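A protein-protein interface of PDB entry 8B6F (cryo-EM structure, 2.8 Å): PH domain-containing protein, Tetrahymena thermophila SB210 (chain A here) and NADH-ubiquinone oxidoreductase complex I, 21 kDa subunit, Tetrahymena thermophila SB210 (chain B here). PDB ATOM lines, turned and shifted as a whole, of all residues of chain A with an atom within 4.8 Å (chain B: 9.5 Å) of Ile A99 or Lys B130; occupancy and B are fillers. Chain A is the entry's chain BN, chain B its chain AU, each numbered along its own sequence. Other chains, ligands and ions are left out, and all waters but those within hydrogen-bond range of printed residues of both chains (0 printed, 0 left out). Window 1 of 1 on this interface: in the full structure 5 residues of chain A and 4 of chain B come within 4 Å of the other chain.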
ATOM      1  N   ARG A  92      34.842 -13.230 -17.871  1.00  0.00           N
ATOM      2  CA  ARG A  92      33.470 -12.786 -18.083  1.00  0.00           C
ATOM      3  C   ARG A  92      32.966 -13.203 -19.456  1.00  0.00           C
ATOM      4  O   ARG A  92      31.777 -13.495 -19.619  1.00  0.00           O
ATOM      5  CB  ARG A  92      33.378 -11.269 -17.932  1.00  0.00           C
ATOM      6  CG  ARG A  92      33.342 -10.775 -16.497  1.00  0.00           C
ATOM      7  CD  ARG A  92      33.267  -9.259 -16.459  1.00  0.00           C
ATOM      8  NE  ARG A  92      32.097  -8.763 -17.172  1.00  0.00           N
ATOM      9  CZ  ARG A  92      31.906  -7.497 -17.518  1.00  0.00           C
ATOM     10  NH1 ARG A  92      32.800  -6.562 -17.241  1.00  0.00           N
ATOM     11  NH2 ARG A  92      30.793  -7.161 -18.160  1.00  0.00           N
ATOM     12  N   ARG A  96      29.298 -16.738 -18.596  1.00  0.00           N
ATOM     13  CA  ARG A  96      28.297 -15.680 -18.568  1.00  0.00           C
ATOM     14  C   ARG A  96      28.522 -14.685 -19.700  1.00  0.00           C
ATOM     15  O   ARG A  96      28.610 -13.478 -19.448  1.00  0.00           O
ATOM     16  CB  ARG A  96      28.323 -14.942 -17.226  1.00  0.00           C
ATOM     17  CG  ARG A  96      28.286 -15.844 -16.004  1.00  0.00           C
ATOM     18  CD  ARG A  96      26.954 -16.559 -15.894  1.00  0.00           C
ATOM     19  NE  ARG A  96      26.890 -17.433 -14.729  1.00  0.00           N
ATOM     20  CZ  ARG A  96      27.381 -18.664 -14.686  1.00  0.00           C
ATOM     21  NH1 ARG A  96      28.013 -19.194 -15.720  1.00  0.00           N
ATOM     22  NH2 ARG A  96      27.234 -19.381 -13.577  1.00  0.00           N
ATOM     23  N   PRO A  97      28.620 -15.137 -20.954  1.00  0.00           N
ATOM     24  CA  PRO A  97      28.813 -14.181 -22.055  1.00  0.00           C
ATOM     25  C   PRO A  97      27.658 -13.212 -22.231  1.00  0.00           C
ATOM     26  O   PRO A  97      27.867 -12.120 -22.770  1.00  0.00           O
ATOM     27  CB  PRO A  97      28.982 -15.087 -23.282  1.00  0.00           C
ATOM     28  CG  PRO A  97      28.332 -16.363 -22.909  1.00  0.00           C
ATOM     29  CD  PRO A  97      28.548 -16.526 -21.437  1.00  0.00           C
ATOM     30  N   GLU A  98      26.447 -13.573 -21.801  1.00  0.00           N
ATOM     31  CA  GLU A  98      25.306 -12.681 -21.981  1.00  0.00           C
ATOM     32  C   GLU A  98      25.487 -11.393 -21.191  1.00  0.00           C
ATOM     33  O   GLU A  98      25.224 -10.299 -21.702  1.00  0.00           O
ATOM     34  CB  GLU A  98      24.014 -13.381 -21.563  1.00  0.00           C
ATOM     35  CG  GLU A  98      23.603 -14.535 -22.457  1.00  0.00           C
ATOM     36  CD  GLU A  98      24.423 -15.787 -22.220  1.00  0.00           C
ATOM     37  OE1 GLU A  98      25.428 -15.713 -21.485  1.00  0.00           O
ATOM     38  OE2 GLU A  98      24.062 -16.850 -22.765  1.00  0.00           O
ATOM     39  N   ILE A  99      25.923 -11.505 -19.936  1.00  0.00           N
ATOM     40  CA  ILE A  99      26.151 -10.317 -19.117  1.00  0.00           C
ATOM     41  C   ILE A  99      27.278  -9.480 -19.704  1.00  0.00           C
ATOM     42  O   ILE A  99      27.224  -8.245 -19.704  1.00  0.00           O
ATOM     43  CB  ILE A  99      26.440 -10.721 -17.660  1.00  0.00           C
ATOM     44  CG1 ILE A  99      25.224 -11.433 -17.063  1.00  0.00           C
ATOM     45  CG2 ILE A  99      26.801  -9.498 -16.822  1.00  0.00           C
ATOM     46  CD1 ILE A  99      25.495 -12.101 -15.735  1.00  0.00           C
ATOM     47  N   PHE A 100      28.322 -10.140 -20.208  1.00  0.00           N
ATOM     48  CA  PHE A 100      29.420  -9.425 -20.849  1.00  0.00           C
ATOM     49  C   PHE A 100      28.914  -8.596 -22.023  1.00  0.00           C
ATOM     50  O   PHE A 100      29.247  -7.413 -22.152  1.00  0.00           O
ATOM     51  CB  PHE A 100      30.483 -10.428 -21.301  1.00  0.00           C
ATOM     52  CG  PHE A 100      31.685  -9.796 -21.940  1.00  0.00           C
ATOM     53  CD1 PHE A 100      32.709  -9.284 -21.162  1.00  0.00           C
ATOM     54  CD2 PHE A 100      31.807  -9.743 -23.318  1.00  0.00           C
ATOM     55  CE1 PHE A 100      33.821  -8.712 -21.746  1.00  0.00           C
ATOM     56  CE2 PHE A 100      32.917  -9.175 -23.907  1.00  0.00           C
ATOM     57  CZ  PHE A 100      33.925  -8.658 -23.119  1.00  0.00           C
ATOM     58  N   LEU A 101      28.110  -9.206 -22.895  1.00  0.00           N
ATOM     59  CA  LEU A 101      27.590  -8.488 -24.054  1.00  0.00           C
ATOM     60  C   LEU A 101      26.663  -7.351 -23.638  1.00  0.00           C
ATOM     61  O   LEU A 101      26.712  -6.260 -24.217  1.00  0.00           O
ATOM     62  CB  LEU A 101      26.862  -9.458 -24.983  1.00  0.00           C
ATOM     63  CG  LEU A 101      27.738 -10.527 -25.641  1.00  0.00           C
ATOM     64  CD1 LEU A 101      26.881 -11.517 -26.405  1.00  0.00           C
ATOM     65  CD2 LEU A 101      28.768  -9.897 -26.561  1.00  0.00           C
ATOM     66  N   ARG A 102      25.807  -7.586 -22.641  1.00  0.00           N
ATOM     67  CA  ARG A 102      24.882  -6.544 -22.206  1.00  0.00           C
ATOM     68  C   ARG A 102      25.627  -5.362 -21.595  1.00  0.00           C
ATOM     69  O   ARG A 102      25.272  -4.206 -21.844  1.00  0.00           O
ATOM     70  CB  ARG A 102      23.865  -7.114 -21.221  1.00  0.00           C
ATOM     71  CG  ARG A 102      22.763  -6.129 -20.864  1.00  0.00           C
ATOM     72  CD  ARG A 102      21.440  -6.824 -20.589  1.00  0.00           C
ATOM     73  NE  ARG A 102      20.945  -7.541 -21.758  1.00  0.00           N
ATOM     74  CZ  ARG A 102      19.777  -8.165 -21.816  1.00  0.00           C
ATOM     75  NH1 ARG A 102      18.943  -8.168 -20.789  1.00  0.00           N
ATOM     76  NH2 ARG A 102      19.440  -8.808 -22.930  1.00  0.00           N
ATOM     77  N   ASP A 103      26.654  -5.629 -20.784  1.00  0.00           N
ATOM     78  CA  ASP A 103      27.474  -4.541 -20.260  1.00  0.00           C
ATOM     79  C   ASP A 103      28.143  -3.777 -21.392  1.00  0.00           C
ATOM     80  O   ASP A 103      28.198  -2.542 -21.377  1.00  0.00           O
ATOM     81  CB  ASP A 103      28.535  -5.086 -19.302  1.00  0.00           C
ATOM     82  CG  ASP A 103      27.941  -5.656 -18.032  1.00  0.00           C
ATOM     83  OD1 ASP A 103      26.912  -5.125 -17.564  1.00  0.00           O
ATOM     84  OD2 ASP A 103      28.500  -6.636 -17.498  1.00  0.00           O
ATOM     85  N   LYS B 127      24.223  -5.158  -3.653  1.00  0.00           N
ATOM     86  CA  LYS B 127      24.819  -5.485  -4.935  1.00  0.00           C
ATOM     87  C   LYS B 127      23.790  -6.141  -5.852  1.00  0.00           C
ATOM     88  O   LYS B 127      22.658  -6.435  -5.459  1.00  0.00           O
ATOM     89  CB  LYS B 127      26.008  -6.426  -4.747  1.00  0.00           C
ATOM     90  CG  LYS B 127      27.090  -5.903  -3.818  1.00  0.00           C
ATOM     91  CD  LYS B 127      28.029  -7.021  -3.377  1.00  0.00           C
ATOM     92  CE  LYS B 127      28.674  -7.721  -4.567  1.00  0.00           C
ATOM     93  NZ  LYS B 127      29.663  -8.750  -4.141  1.00  0.00           N
ATOM     94  N   LEU B 128      24.201  -6.361  -7.096  1.00  0.00           N
ATOM     95  CA  LEU B 128      23.471  -7.193  -8.043  1.00  0.00           C
ATOM     96  C   LEU B 128      24.331  -8.421  -8.306  1.00  0.00           C
ATOM     97  O   LEU B 128      25.419  -8.312  -8.882  1.00  0.00           O
ATOM     98  CB  LEU B 128      23.163  -6.436  -9.333  1.00  0.00           C
ATOM     99  CG  LEU B 128      21.983  -5.460  -9.271  1.00  0.00           C
ATOM    100  CD1 LEU B 128      21.911  -4.625 -10.535  1.00  0.00           C
ATOM    101  CD2 LEU B 128      20.669  -6.195  -9.055  1.00  0.00           C
ATOM    102  N   ASN B 129      23.849  -9.586  -7.880  1.00  0.00           N
ATOM    103  CA  ASN B 129      24.630 -10.808  -7.992  1.00  0.00           C
ATOM    104  C   ASN B 129      24.650 -11.278  -9.440  1.00  0.00           C
ATOM    105  O   ASN B 129      24.069 -12.315  -9.776  1.00  0.00           O
ATOM    106  CB  ASN B 129      24.055 -11.889  -7.074  1.00  0.00           C
ATOM    107  CG  ASN B 129      25.018 -13.034  -6.844  1.00  0.00           C
ATOM    108  OD1 ASN B 129      26.224 -12.897  -7.045  1.00  0.00           O
ATOM    109  ND2 ASN B 129      24.488 -14.174  -6.416  1.00  0.00           N
ATOM    110  N   LYS B 130      25.320 -10.513 -10.305  1.00  0.00           N
ATOM    111  CA  LYS B 130      25.333 -10.840 -11.725  1.00  0.00           C
ATOM    112  C   LYS B 130      26.028 -12.170 -11.984  1.00  0.00           C
ATOM    113  O   LYS B 130      25.531 -13.000 -12.750  1.00  0.00           O
ATOM    114  CB  LYS B 130      26.012  -9.718 -12.510  1.00  0.00           C
ATOM    115  CG  LYS B 130      25.346  -8.365 -12.327  1.00  0.00           C
ATOM    116  CD  LYS B 130      25.875  -7.339 -13.308  1.00  0.00           C
ATOM    117  CE  LYS B 130      27.345  -7.056 -13.078  1.00  0.00           C
ATOM    118  NZ  LYS B 130      27.847  -5.986 -13.983  1.00  0.00           N
ATOM    119  N   TYR B 131      27.175 -12.390 -11.350  1.00  0.00           N
ATOM    120  CA  TYR B 131      27.927 -13.630 -11.490  1.00  0.00           C
ATOM    121  C   TYR B 131      27.718 -14.455 -10.229  1.00  0.00           C
ATOM    122  O   TYR B 131      28.048 -14.005  -9.128  1.00  0.00           O
ATOM    123  CB  TYR B 131      29.410 -13.340 -11.715  1.00  0.00           C
ATOM    124  CG  TYR B 131      29.655 -12.197 -12.671  1.00  0.00           C
ATOM    125  CD1 TYR B 131      29.489 -12.361 -14.038  1.00  0.00           C
ATOM    126  CD2 TYR B 131      30.056 -10.954 -12.206  1.00  0.00           C
ATOM    127  CE1 TYR B 131      29.710 -11.319 -14.914  1.00  0.00           C
ATOM    128  CE2 TYR B 131      30.279  -9.907 -13.071  1.00  0.00           C
ATOM    129  CZ  TYR B 131      30.106 -10.096 -14.425  1.00  0.00           C
ATOM    130  OH  TYR B 131      30.329  -9.053 -15.294  1.00  0.00           O
ATOM    131  N   ASP B 132      27.174 -15.660 -10.391  1.00  0.00           N
ATOM    132  CA  ASP B 132      26.766 -16.485  -9.255  1.00  0.00           C
ATOM    133  C   ASP B 132      27.110 -17.938  -9.566  1.00  0.00           C
ATOM    134  O   ASP B 132      26.330 -18.639 -10.216  1.00  0.00           O
ATOM    135  CB  ASP B 132      25.279 -16.315  -8.974  1.00  0.00           C
ATOM    136  CG  ASP B 132      24.832 -17.061  -7.739  1.00  0.00           C
ATOM    137  OD1 ASP B 132      25.695 -17.638  -7.046  1.00  0.00           O
ATOM    138  OD2 ASP B 132      23.616 -17.070  -7.461  1.00  0.00           O
ATOM    139  N   PHE B 133      28.273 -18.384  -9.101  1.00  0.00           N
ATOM    140  CA  PHE B 133      28.682 -19.775  -9.228  1.00  0.00           C
ATOM    141  C   PHE B 133      28.573 -20.548  -7.920  1.00  0.00           C
ATOM    142  O   PHE B 133      28.870 -21.746  -7.901  1.00  0.00           O
ATOM    143  CB  PHE B 133      30.125 -19.856  -9.736  1.00  0.00           C
ATOM    144  CG  PHE B 133      30.365 -19.104 -11.010  1.00  0.00           C
ATOM    145  CD1 PHE B 133      30.762 -17.778 -10.984  1.00  0.00           C
ATOM    146  CD2 PHE B 133      30.207 -19.729 -12.233  1.00  0.00           C
ATOM    147  CE1 PHE B 133      30.989 -17.089 -12.156  1.00  0.00           C
ATOM    148  CE2 PHE B 133      30.431 -19.044 -13.408  1.00  0.00           C
ATOM    149  CZ  PHE B 133      30.824 -17.722 -13.369  1.00  0.00           C
ATOM    150  N   THR B 134      28.155 -19.900  -6.832  1.00  0.00           N
ATOM    151  CA  THR B 134      28.218 -20.503  -5.508  1.00  0.00           C
ATOM    152  C   THR B 134      26.926 -20.443  -4.706  1.00  0.00           C
ATOM    153  O   THR B 134      26.858 -21.085  -3.653  1.00  0.00           O
ATOM    154  CB  THR B 134      29.332 -19.843  -4.683  1.00  0.00           C
ATOM    155  OG1 THR B 134      29.177 -18.424  -4.726  1.00  0.00           O
ATOM    156  CG2 THR B 134      30.696 -20.213  -5.221  1.00  0.00           C
ATOM    157  N   SER B 135      25.902 -19.715  -5.156  1.00  0.00           N
ATOM    158  CA  SER B 135      24.687 -19.598  -4.354  1.00  0.00           C
ATOM    159  C   SER B 135      24.028 -20.958  -4.175  1.00  0.00           C
ATOM    160  O   SER B 135      23.745 -21.380  -3.048  1.00  0.00           O
ATOM    161  CB  SER B 135      23.718 -18.608  -5.000  1.00  0.00           C
ATOM    162  OG  SER B 135      23.308 -19.058  -6.279  1.00  0.00           O
ATOM    163  N   ARG B 149      26.023 -13.197   3.262  1.00  0.00           N
ATOM    164  CA  ARG B 149      25.316 -12.613   2.133  1.00  0.00           C
ATOM    165  C   ARG B 149      24.366 -11.533   2.627  1.00  0.00           C
ATOM    166  O   ARG B 149      23.656 -11.723   3.620  1.00  0.00           O
ATOM    167  CB  ARG B 149      24.542 -13.679   1.354  1.00  0.00           C
ATOM    168  CG  ARG B 149      25.436 -14.700   0.670  1.00  0.00           C
ATOM    169  CD  ARG B 149      24.631 -15.660  -0.190  1.00  0.00           C
ATOM    170  NE  ARG B 149      25.493 -16.552  -0.954  1.00  0.00           N
ATOM    171  CZ  ARG B 149      26.035 -16.253  -2.127  1.00  0.00           C
ATOM    172  NH1 ARG B 149      25.830 -15.082  -2.707  1.00  0.00           N
ATOM    173  NH2 ARG B 149      26.806 -17.151  -2.734  1.00  0.00           N
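Of the 9 printed residues of chain A, 4 touch a printed residue of chain B.
Hydrophobic or aromatic side chains of chain A that line the printed part of chain B: Ile A99.
Along chain A the printed residues that touch a printed residue of chain B span positions 92 to 103.
Of the 10 printed residues of chain B, 4 touch a printed residue of chain A.
Hydrophobic or aromatic side chains of chain B within 4 Å of the printed part of chain A: Tyr B131 and Phe B133.
Among the printed residues, 7 pairs touch across the chains.
The backbone carbonyl oxygen of Tyr B131 sits close to the side-chain amide oxygen of Asn B129 (3.0 Å).
The side-chain carboxylate (OD2) of Asp B132 lies close to the side-chain amide nitrogen (ND2) of Asn B129, at 3.2 Å.
N of Thr B134 is in hydrogen-bond range of OD1 of Asp B132 (3.3 Å).
The side-chain carboxylate (OD1) of Asp B132 sits at hydrogen-bond distance from the backbone NH (N) of Ser B135 (2.8 Å).
The guanidinium group (NH2) of Arg A92 is in salt-bridge range of the side-chain carboxylate (OD2) of Asp A103.
Among the printed residues, merely in contact across the chains: Arg A96 with Asp B132 (3.6 Å), Arg A96 with Phe B133 (3.2 Å), Ile A99 with Lys B130 (3.1 Å), Ile A99 with Tyr B131 (3.9 Å) and Asp A103 with Tyr B131 (3.7 Å).
Ile A99 touches just these residues of chain B: Lys B130 and Tyr B131.
Lys B130 touches just these residues of chain A: Ile A99 and Asp A103.
Of the printed residues of chain B, Arg A96 touches Asp B132 and Phe B133.
Printed residues of chain A within 4 Å of Phe B133: Arg A96 (3.2 Å).
Of the printed residues of chain B, Asp A103 touches Lys B130 and Tyr B131.
Printed residues of chain A within 4 Å of Asp B132: Arg A96 (3.6 Å).
Leu B128 touches none of the printed residues of chain A.
Arg A102 touches none of the printed residues of chain B.
The nearest residue of chain B that does not touch Ile A99 is Asn B129 (6.1 Å).
The nearest printed residue of chain A that does not touch Lys B130 is Arg A96 (5.0 Å).
The nearest printed residue of chain A that does not touch Asp B132 is Ile A99 (6.6 Å).
OD2 of Asp A103 lies within salt-bridge range of NZ of Lys B130.
The guanidinium group of Arg A92 lies within hydrogen-bond range of the side-chain hydroxyl of Tyr B131 (2.6 Å).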
